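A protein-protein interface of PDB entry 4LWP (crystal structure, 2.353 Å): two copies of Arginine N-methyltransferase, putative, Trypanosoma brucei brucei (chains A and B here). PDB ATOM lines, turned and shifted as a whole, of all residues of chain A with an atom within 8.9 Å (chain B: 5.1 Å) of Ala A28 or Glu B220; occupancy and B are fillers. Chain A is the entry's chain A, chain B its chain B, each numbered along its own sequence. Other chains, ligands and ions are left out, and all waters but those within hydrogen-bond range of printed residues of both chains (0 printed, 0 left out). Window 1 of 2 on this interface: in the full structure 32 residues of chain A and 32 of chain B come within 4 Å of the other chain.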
ATOM      1  N   ASP A  26       7.129  19.824  -2.506  1.00  0.00           N
ATOM      2  CA  ASP A  26       8.543  20.144  -2.353  1.00  0.00           C
ATOM      3  C   ASP A  26       9.408  19.409  -3.379  1.00  0.00           C
ATOM      4  O   ASP A  26       9.682  18.211  -3.250  1.00  0.00           O
ATOM      5  CB  ASP A  26       9.022  19.810  -0.945  1.00  0.00           C
ATOM      6  CG  ASP A  26      10.408  20.351  -0.669  1.00  0.00           C
ATOM      7  OD1 ASP A  26      10.536  21.578  -0.443  1.00  0.00           O
ATOM      8  OD2 ASP A  26      11.374  19.556  -0.689  1.00  0.00           O
ATOM      9  N   LEU A  27       9.846  20.151  -4.387  1.00  0.00           N
ATOM     10  CA  LEU A  27      10.593  19.598  -5.499  1.00  0.00           C
ATOM     11  C   LEU A  27      11.979  19.067  -5.145  1.00  0.00           C
ATOM     12  O   LEU A  27      12.549  18.276  -5.898  1.00  0.00           O
ATOM     13  CB  LEU A  27      10.709  20.656  -6.575  1.00  0.00           C
ATOM     14  CG  LEU A  27       9.388  20.795  -7.323  1.00  0.00           C
ATOM     15  CD1 LEU A  27       9.453  21.990  -8.231  1.00  0.00           C
ATOM     16  CD2 LEU A  27       9.100  19.552  -8.116  1.00  0.00           C
ATOM     17  N   ALA A  28      12.537  19.502  -4.022  1.00  0.00           N
ATOM     18  CA  ALA A  28      13.848  19.003  -3.619  1.00  0.00           C
ATOM     19  C   ALA A  28      13.753  17.530  -3.226  1.00  0.00           C
ATOM     20  O   ALA A  28      14.645  16.724  -3.523  1.00  0.00           O
ATOM     21  CB  ALA A  28      14.411  19.829  -2.455  1.00  0.00           C
ATOM     22  N   VAL A  29      12.663  17.165  -2.569  1.00  0.00           N
ATOM     23  CA  VAL A  29      12.469  15.763  -2.241  1.00  0.00           C
ATOM     24  C   VAL A  29      12.266  14.982  -3.546  1.00  0.00           C
ATOM     25  O   VAL A  29      12.781  13.871  -3.689  1.00  0.00           O
ATOM     26  CB  VAL A  29      11.274  15.561  -1.270  1.00  0.00           C
ATOM     27  CG1 VAL A  29      10.958  14.068  -1.060  1.00  0.00           C
ATOM     28  CG2 VAL A  29      11.567  16.236   0.064  1.00  0.00           C
ATOM     29  N   HIS A  30      11.576  15.573  -4.523  1.00  0.00           N
ATOM     30  CA  HIS A  30      11.376  14.868  -5.788  1.00  0.00           C
ATOM     31  C   HIS A  30      12.671  14.696  -6.559  1.00  0.00           C
ATOM     32  O   HIS A  30      12.864  13.639  -7.159  1.00  0.00           O
ATOM     33  CB  HIS A  30      10.331  15.576  -6.655  1.00  0.00           C
ATOM     34  CG  HIS A  30       8.923  15.372  -6.173  1.00  0.00           C
ATOM     35  ND1 HIS A  30       8.112  14.358  -6.643  1.00  0.00           N
ATOM     36  CD2 HIS A  30       8.193  16.035  -5.242  1.00  0.00           C
ATOM     37  CE1 HIS A  30       6.942  14.410  -6.026  1.00  0.00           C
ATOM     38  NE2 HIS A  30       6.967  15.416  -5.168  1.00  0.00           N
ATOM     39  N   ARG A  31      13.574  15.686  -6.526  1.00  0.00           N
ATOM     40  CA  ARG A  31      14.844  15.516  -7.219  1.00  0.00           C
ATOM     41  C   ARG A  31      15.596  14.309  -6.669  1.00  0.00           C
ATOM     42  O   ARG A  31      16.155  13.514  -7.417  1.00  0.00           O
ATOM     43  CB  ARG A  31      15.778  16.734  -7.086  1.00  0.00           C
ATOM     44  CG  ARG A  31      17.075  16.444  -7.869  1.00  0.00           C
ATOM     45  CD  ARG A  31      18.297  17.334  -7.599  1.00  0.00           C
ATOM     46  NE  ARG A  31      18.206  18.698  -8.083  1.00  0.00           N
ATOM     47  CZ  ARG A  31      19.218  19.364  -8.624  1.00  0.00           C
ATOM     48  NH1 ARG A  31      20.398  18.785  -8.791  1.00  0.00           N
ATOM     49  NH2 ARG A  31      19.034  20.611  -9.005  1.00  0.00           N
ATOM     50  N   LEU A  32      15.605  14.210  -5.346  1.00  0.00           N
ATOM     51  CA  LEU A  32      16.192  13.092  -4.616  1.00  0.00           C
ATOM     52  C   LEU A  32      15.651  11.747  -5.115  1.00  0.00           C
ATOM     53  O   LEU A  32      16.417  10.806  -5.332  1.00  0.00           O
ATOM     54  CB  LEU A  32      15.911  13.271  -3.118  1.00  0.00           C
ATOM     55  CG  LEU A  32      16.485  12.336  -2.056  1.00  0.00           C
ATOM     56  CD1 LEU A  32      17.978  12.528  -1.914  1.00  0.00           C
ATOM     57  CD2 LEU A  32      15.782  12.561  -0.722  1.00  0.00           C
ATOM     58  N   MET A  33      14.336  11.663  -5.310  1.00  0.00           N
ATOM     59  CA  MET A  33      13.739  10.427  -5.817  1.00  0.00           C
ATOM     60  C   MET A  33      14.065  10.222  -7.302  1.00  0.00           C
ATOM     61  O   MET A  33      14.213   9.092  -7.744  1.00  0.00           O
ATOM     62  CB  MET A  33      12.227  10.426  -5.591  1.00  0.00           C
ATOM     63  CG  MET A  33      11.813  10.420  -4.109  1.00  0.00           C
ATOM     64  SD  MET A  33      10.005  10.250  -3.881  1.00  0.00           S
ATOM     65  CE  MET A  33       9.409  11.582  -4.919  1.00  0.00           C
ATOM     66  N   LEU A  34      14.181  11.312  -8.061  1.00  0.00           N
ATOM     67  CA  LEU A  34      14.548  11.219  -9.478  1.00  0.00           C
ATOM     68  C   LEU A  34      16.047  10.919  -9.682  1.00  0.00           C
ATOM     69  O   LEU A  34      16.455  10.408 -10.734  1.00  0.00           O
ATOM     70  CB  LEU A  34      14.170  12.507 -10.216  1.00  0.00           C
ATOM     71  CG  LEU A  34      12.671  12.833 -10.320  1.00  0.00           C
ATOM     72  CD1 LEU A  34      12.435  14.223 -10.887  1.00  0.00           C
ATOM     73  CD2 LEU A  34      11.954  11.794 -11.148  1.00  0.00           C
ATOM     74  N   GLU A  35      16.846  11.229  -8.665  1.00  0.00           N
ATOM     75  CA  GLU A  35      18.276  10.950  -8.660  1.00  0.00           C
ATOM     76  C   GLU A  35      18.635   9.547  -8.165  1.00  0.00           C
ATOM     77  O   GLU A  35      19.796   9.139  -8.242  1.00  0.00           O
ATOM     78  CB  GLU A  35      19.007  11.981  -7.801  1.00  0.00           C
ATOM     79  CG  GLU A  35      19.170  13.331  -8.490  1.00  0.00           C
ATOM     80  CD  GLU A  35      19.920  14.355  -7.643  1.00  0.00           C
ATOM     81  OE1 GLU A  35      19.809  14.295  -6.390  1.00  0.00           O
ATOM     82  OE2 GLU A  35      20.623  15.218  -8.244  1.00  0.00           O
ATOM     83  N   THR A  65       5.883  14.555 -10.152  1.00  0.00           N
ATOM     84  CA  THR A  65       6.406  15.222 -11.341  1.00  0.00           C
ATOM     85  C   THR A  65       5.768  14.663 -12.600  1.00  0.00           C
ATOM     86  O   THR A  65       5.778  15.301 -13.655  1.00  0.00           O
ATOM     87  CB  THR A  65       7.950  15.075 -11.455  1.00  0.00           C
ATOM     88  OG1 THR A  65       8.303  13.680 -11.479  1.00  0.00           O
ATOM     89  CG2 THR A  65       8.645  15.744 -10.281  1.00  0.00           C
ATOM     90  N   LEU A  88       1.771  20.655  -7.249  1.00  0.00           N
ATOM     91  CA  LEU A  88       2.623  20.155  -8.318  1.00  0.00           C
ATOM     92  C   LEU A  88       1.801  19.773  -9.537  1.00  0.00           C
ATOM     93  O   LEU A  88       2.285  19.835 -10.661  1.00  0.00           O
ATOM     94  CB  LEU A  88       3.410  18.932  -7.842  1.00  0.00           C
ATOM     95  CG  LEU A  88       4.896  19.086  -7.539  1.00  0.00           C
ATOM     96  CD1 LEU A  88       5.503  17.745  -7.127  1.00  0.00           C
ATOM     97  CD2 LEU A  88       5.618  19.666  -8.746  1.00  0.00           C
ATOM     98  N   PHE A  91       1.615  22.423 -12.195  1.00  0.00           N
ATOM     99  CA  PHE A  91       2.842  22.513 -12.990  1.00  0.00           C
ATOM    100  C   PHE A  91       3.054  21.273 -13.834  1.00  0.00           C
ATOM    101  O   PHE A  91       3.604  21.379 -14.926  1.00  0.00           O
ATOM    102  CB  PHE A  91       4.058  22.759 -12.104  1.00  0.00           C
ATOM    103  CG  PHE A  91       3.955  24.016 -11.285  1.00  0.00           C
ATOM    104  CD1 PHE A  91       4.029  25.258 -11.900  1.00  0.00           C
ATOM    105  CD2 PHE A  91       3.779  23.962  -9.910  1.00  0.00           C
ATOM    106  CE1 PHE A  91       3.929  26.430 -11.160  1.00  0.00           C
ATOM    107  CE2 PHE A  91       3.682  25.126  -9.157  1.00  0.00           C
ATOM    108  CZ  PHE A  91       3.751  26.362  -9.781  1.00  0.00           C
ATOM    109  N   TYR B 201      20.645  23.532 -10.807  1.00  0.00           N
ATOM    110  CA  TYR B 201      19.223  23.267 -11.050  1.00  0.00           C
ATOM    111  C   TYR B 201      18.910  22.870 -12.482  1.00  0.00           C
ATOM    112  O   TYR B 201      18.402  21.773 -12.737  1.00  0.00           O
ATOM    113  CB  TYR B 201      18.371  24.496 -10.676  1.00  0.00           C
ATOM    114  CG  TYR B 201      18.467  24.835  -9.213  1.00  0.00           C
ATOM    115  CD1 TYR B 201      19.475  25.671  -8.750  1.00  0.00           C
ATOM    116  CD2 TYR B 201      17.582  24.292  -8.287  1.00  0.00           C
ATOM    117  CE1 TYR B 201      19.593  25.975  -7.421  1.00  0.00           C
ATOM    118  CE2 TYR B 201      17.690  24.600  -6.938  1.00  0.00           C
ATOM    119  CZ  TYR B 201      18.705  25.445  -6.513  1.00  0.00           C
ATOM    120  OH  TYR B 201      18.858  25.775  -5.176  1.00  0.00           O
ATOM    121  N   TRP B 205      17.417  19.380 -14.234  1.00  0.00           N
ATOM    122  CA  TRP B 205      15.998  19.296 -14.577  1.00  0.00           C
ATOM    123  C   TRP B 205      15.712  19.354 -16.067  1.00  0.00           C
ATOM    124  O   TRP B 205      14.626  18.985 -16.499  1.00  0.00           O
ATOM    125  CB  TRP B 205      15.222  20.421 -13.892  1.00  0.00           C
ATOM    126  CG  TRP B 205      15.058  20.273 -12.413  1.00  0.00           C
ATOM    127  CD1 TRP B 205      15.720  20.963 -11.447  1.00  0.00           C
ATOM    128  CD2 TRP B 205      14.156  19.390 -11.733  1.00  0.00           C
ATOM    129  NE1 TRP B 205      15.298  20.561 -10.209  1.00  0.00           N
ATOM    130  CE2 TRP B 205      14.332  19.601 -10.354  1.00  0.00           C
ATOM    131  CE3 TRP B 205      13.218  18.444 -12.160  1.00  0.00           C
ATOM    132  CZ2 TRP B 205      13.602  18.902  -9.394  1.00  0.00           C
ATOM    133  CZ3 TRP B 205      12.499  17.742 -11.207  1.00  0.00           C
ATOM    134  CH2 TRP B 205      12.694  17.973  -9.840  1.00  0.00           C
ATOM    135  N   TYR B 216      10.121  22.519 -13.596  1.00  0.00           N
ATOM    136  CA  TYR B 216      10.292  22.148 -12.197  1.00  0.00           C
ATOM    137  C   TYR B 216      11.567  22.797 -11.609  1.00  0.00           C
ATOM    138  O   TYR B 216      11.605  23.150 -10.423  1.00  0.00           O
ATOM    139  CB  TYR B 216      10.349  20.613 -12.057  1.00  0.00           C
ATOM    140  CG  TYR B 216       9.053  19.878 -12.419  1.00  0.00           C
ATOM    141  CD1 TYR B 216       7.816  20.315 -11.948  1.00  0.00           C
ATOM    142  CD2 TYR B 216       9.075  18.761 -13.260  1.00  0.00           C
ATOM    143  CE1 TYR B 216       6.642  19.661 -12.288  1.00  0.00           C
ATOM    144  CE2 TYR B 216       7.896  18.095 -13.611  1.00  0.00           C
ATOM    145  CZ  TYR B 216       6.688  18.555 -13.119  1.00  0.00           C
ATOM    146  OH  TYR B 216       5.524  17.909 -13.452  1.00  0.00           O
ATOM    147  N   GLY B 217      12.604  22.926 -12.439  1.00  0.00           N
ATOM    148  CA  GLY B 217      13.840  23.589 -12.053  1.00  0.00           C
ATOM    149  C   GLY B 217      13.679  25.057 -11.678  1.00  0.00           C
ATOM    150  O   GLY B 217      14.230  25.512 -10.668  1.00  0.00           O
ATOM    151  N   ARG B 218      12.921  25.798 -12.481  1.00  0.00           N
ATOM    152  CA  ARG B 218      12.646  27.193 -12.178  1.00  0.00           C
ATOM    153  C   ARG B 218      11.942  27.269 -10.824  1.00  0.00           C
ATOM    154  O   ARG B 218      12.285  28.110  -9.988  1.00  0.00           O
ATOM    155  CB  ARG B 218      11.795  27.848 -13.278  1.00  0.00           C
ATOM    156  CG  ARG B 218      12.490  27.930 -14.653  1.00  0.00           C
ATOM    157  CD  ARG B 218      11.664  28.735 -15.674  1.00  0.00           C
ATOM    158  NE  ARG B 218      10.915  27.894 -16.616  1.00  0.00           N
ATOM    159  CZ  ARG B 218      11.410  27.303 -17.709  1.00  0.00           C
ATOM    160  NH1 ARG B 218      12.686  27.471 -18.077  1.00  0.00           N
ATOM    161  NH2 ARG B 218      10.603  26.563 -18.465  1.00  0.00           N
ATOM    162  N   ILE B 219      10.985  26.369 -10.591  1.00  0.00           N
ATOM    163  CA  ILE B 219      10.263  26.374  -9.319  1.00  0.00           C
ATOM    164  C   ILE B 219      11.156  26.090  -8.110  1.00  0.00           C
ATOM    165  O   ILE B 219      11.156  26.865  -7.158  1.00  0.00           O
ATOM    166  CB  ILE B 219       9.119  25.346  -9.296  1.00  0.00           C
ATOM    167  CG1 ILE B 219       8.100  25.621 -10.399  1.00  0.00           C
ATOM    168  CG2 ILE B 219       8.427  25.386  -7.949  1.00  0.00           C
ATOM    169  CD1 ILE B 219       7.220  26.818 -10.116  1.00  0.00           C
ATOM    170  N   GLU B 220      11.917  24.990  -8.154  1.00  0.00           N
ATOM    171  CA  GLU B 220      12.774  24.572  -7.031  1.00  0.00           C
ATOM    172  C   GLU B 220      13.736  25.699  -6.668  1.00  0.00           C
ATOM    173  O   GLU B 220      13.974  25.983  -5.498  1.00  0.00           O
ATOM    174  CB  GLU B 220      13.573  23.291  -7.364  1.00  0.00           C
ATOM    175  CG  GLU B 220      14.165  22.603  -6.113  1.00  0.00           C
ATOM    176  CD  GLU B 220      15.411  21.752  -6.369  1.00  0.00           C
ATOM    177  OE1 GLU B 220      15.762  21.497  -7.549  1.00  0.00           O
ATOM    178  OE2 GLU B 220      16.047  21.324  -5.369  1.00  0.00           O
ATOM    179  N   TYR B 221      14.269  26.338  -7.701  1.00  0.00           N
ATOM    180  CA  TYR B 221      15.215  27.424  -7.559  1.00  0.00           C
ATOM    181  C   TYR B 221      14.580  28.663  -6.925  1.00  0.00           C
ATOM    182  O   TYR B 221      15.065  29.156  -5.894  1.00  0.00           O
ATOM    183  CB  TYR B 221      15.809  27.747  -8.927  1.00  0.00           C
ATOM    184  CG  TYR B 221      16.662  28.984  -8.979  1.00  0.00           C
ATOM    185  CD1 TYR B 221      17.918  29.013  -8.393  1.00  0.00           C
ATOM    186  CD2 TYR B 221      16.216  30.122  -9.643  1.00  0.00           C
ATOM    187  CE1 TYR B 221      18.699  30.149  -8.455  1.00  0.00           C
ATOM    188  CE2 TYR B 221      16.990  31.255  -9.713  1.00  0.00           C
ATOM    189  CZ  TYR B 221      18.228  31.264  -9.119  1.00  0.00           C
ATOM    190  OH  TYR B 221      18.984  32.407  -9.189  1.00  0.00           O
ATOM    191  N   GLU B 222      13.493  29.150  -7.524  1.00  0.00           N
ATOM    192  CA  GLU B 222      12.832  30.355  -7.025  1.00  0.00           C
ATOM    193  C   GLU B 222      12.458  30.231  -5.550  1.00  0.00           C
ATOM    194  O   GLU B 222      12.598  31.192  -4.794  1.00  0.00           O
ATOM    195  CB  GLU B 222      11.584  30.674  -7.850  1.00  0.00           C
ATOM    196  N   VAL B 223      12.004  29.056  -5.129  1.00  0.00           N
ATOM    197  CA  VAL B 223      11.578  28.908  -3.742  1.00  0.00           C
ATOM    198  C   VAL B 223      12.754  28.734  -2.786  1.00  0.00           C
ATOM    199  O   VAL B 223      12.648  29.089  -1.614  1.00  0.00           O
ATOM    200  CB  VAL B 223      10.595  27.719  -3.539  1.00  0.00           C
ATOM    201  CG1 VAL B 223       9.485  27.754  -4.579  1.00  0.00           C
ATOM    202  CG2 VAL B 223      11.323  26.387  -3.579  1.00  0.00           C
ATOM    203  N   TYR B 224      13.883  28.214  -3.258  1.00  0.00           N
ATOM    204  CA  TYR B 224      14.999  28.029  -2.330  1.00  0.00           C
ATOM    205  C   TYR B 224      15.655  29.381  -2.025  1.00  0.00           C
ATOM    206  O   TYR B 224      16.189  29.572  -0.939  1.00  0.00           O
ATOM    207  CB  TYR B 224      16.023  27.023  -2.868  1.00  0.00           C
ATOM    208  CG  TYR B 224      17.215  26.821  -1.948  1.00  0.00           C
ATOM    209  CD1 TYR B 224      17.109  26.065  -0.781  1.00  0.00           C
ATOM    210  CD2 TYR B 224      18.448  27.393  -2.242  1.00  0.00           C
ATOM    211  CE1 TYR B 224      18.205  25.887   0.070  1.00  0.00           C
ATOM    212  CE2 TYR B 224      19.548  27.211  -1.404  1.00  0.00           C
ATOM    213  CZ  TYR B 224      19.421  26.470  -0.251  1.00  0.00           C
ATOM    214  OH  TYR B 224      20.518  26.312   0.572  1.00  0.00           O
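Of chain B, only Glu B220 (3.6 Å) comes within 4 Å of Ala A28.
Of chain A, only Leu A27 (3.9 Å), Ala A28 (3.6 Å) and Arg A31 (3.7 Å) come within 4 Å of Glu B220.
Printed residues of chain B within 4 Å of Leu A88: Tyr B216 (3.7 Å).
Printed residues of chain B within 4 Å of Phe A91: Ile B219 (3.5 Å).
Of the printed residues of chain A, Tyr B216 touches Leu A27, Thr A65 and Leu A88.
Of the printed residues of chain A, Tyr B201 touches Arg A31.
Val B223 touches none of the printed residues of chain A.
Tyr B224 touches none of the printed residues of chain A.
The nearest printed residue of chain B that does not touch Ala A28 is Trp B205 (5.5 Å).
The nearest residue of chain A that does not touch Glu B220 is Val A29 (6.0 Å).
The indole nitrogen of Trp B205 is in hydrogen-bond range of the side-chain carboxylate of Glu B220 (2.9 Å).
The guanidinium group (NH1) of Arg A31 is in salt-bridge range of the side-chain carboxylate (OE2) of Glu A35, at 3.6 Å.
Among the printed residues, pairs that only touch across the chains: Leu A27 with Tyr B216, Arg A31 with Tyr B201, Phe A91 with Ile B219, Leu A34 with Trp B205, Leu A27 with Ile B219, Ala A28 with Glu B220, Leu A88 with Tyr B216, Leu A27 with Trp B205, Arg A31 with Trp B205 and Leu A27 with Glu B220.
OE1 of Glu B220 is in salt-bridge range of NH2 of Arg A31.
The side-chain hydroxyl (OH) of Tyr B216 lies within hydrogen-bond range of the backbone carbonyl oxygen (O) of Thr A65, at 2.6 Å.
Of the 11 printed residues of chain B, 5 touch a printed residue of chain A.
Among the printed residues, 12 pairs touch across the chains.
Among the printed residues, Asp or Glu carboxylates within 4 Å of a Lys or Arg side-chain nitrogen of the other chain: Arg A31 with Glu B220.
No position is printed for both chains.
Of the 12 pairs that touch across the chains among the printed residues, none has its exchanged pair printed and touching as well.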
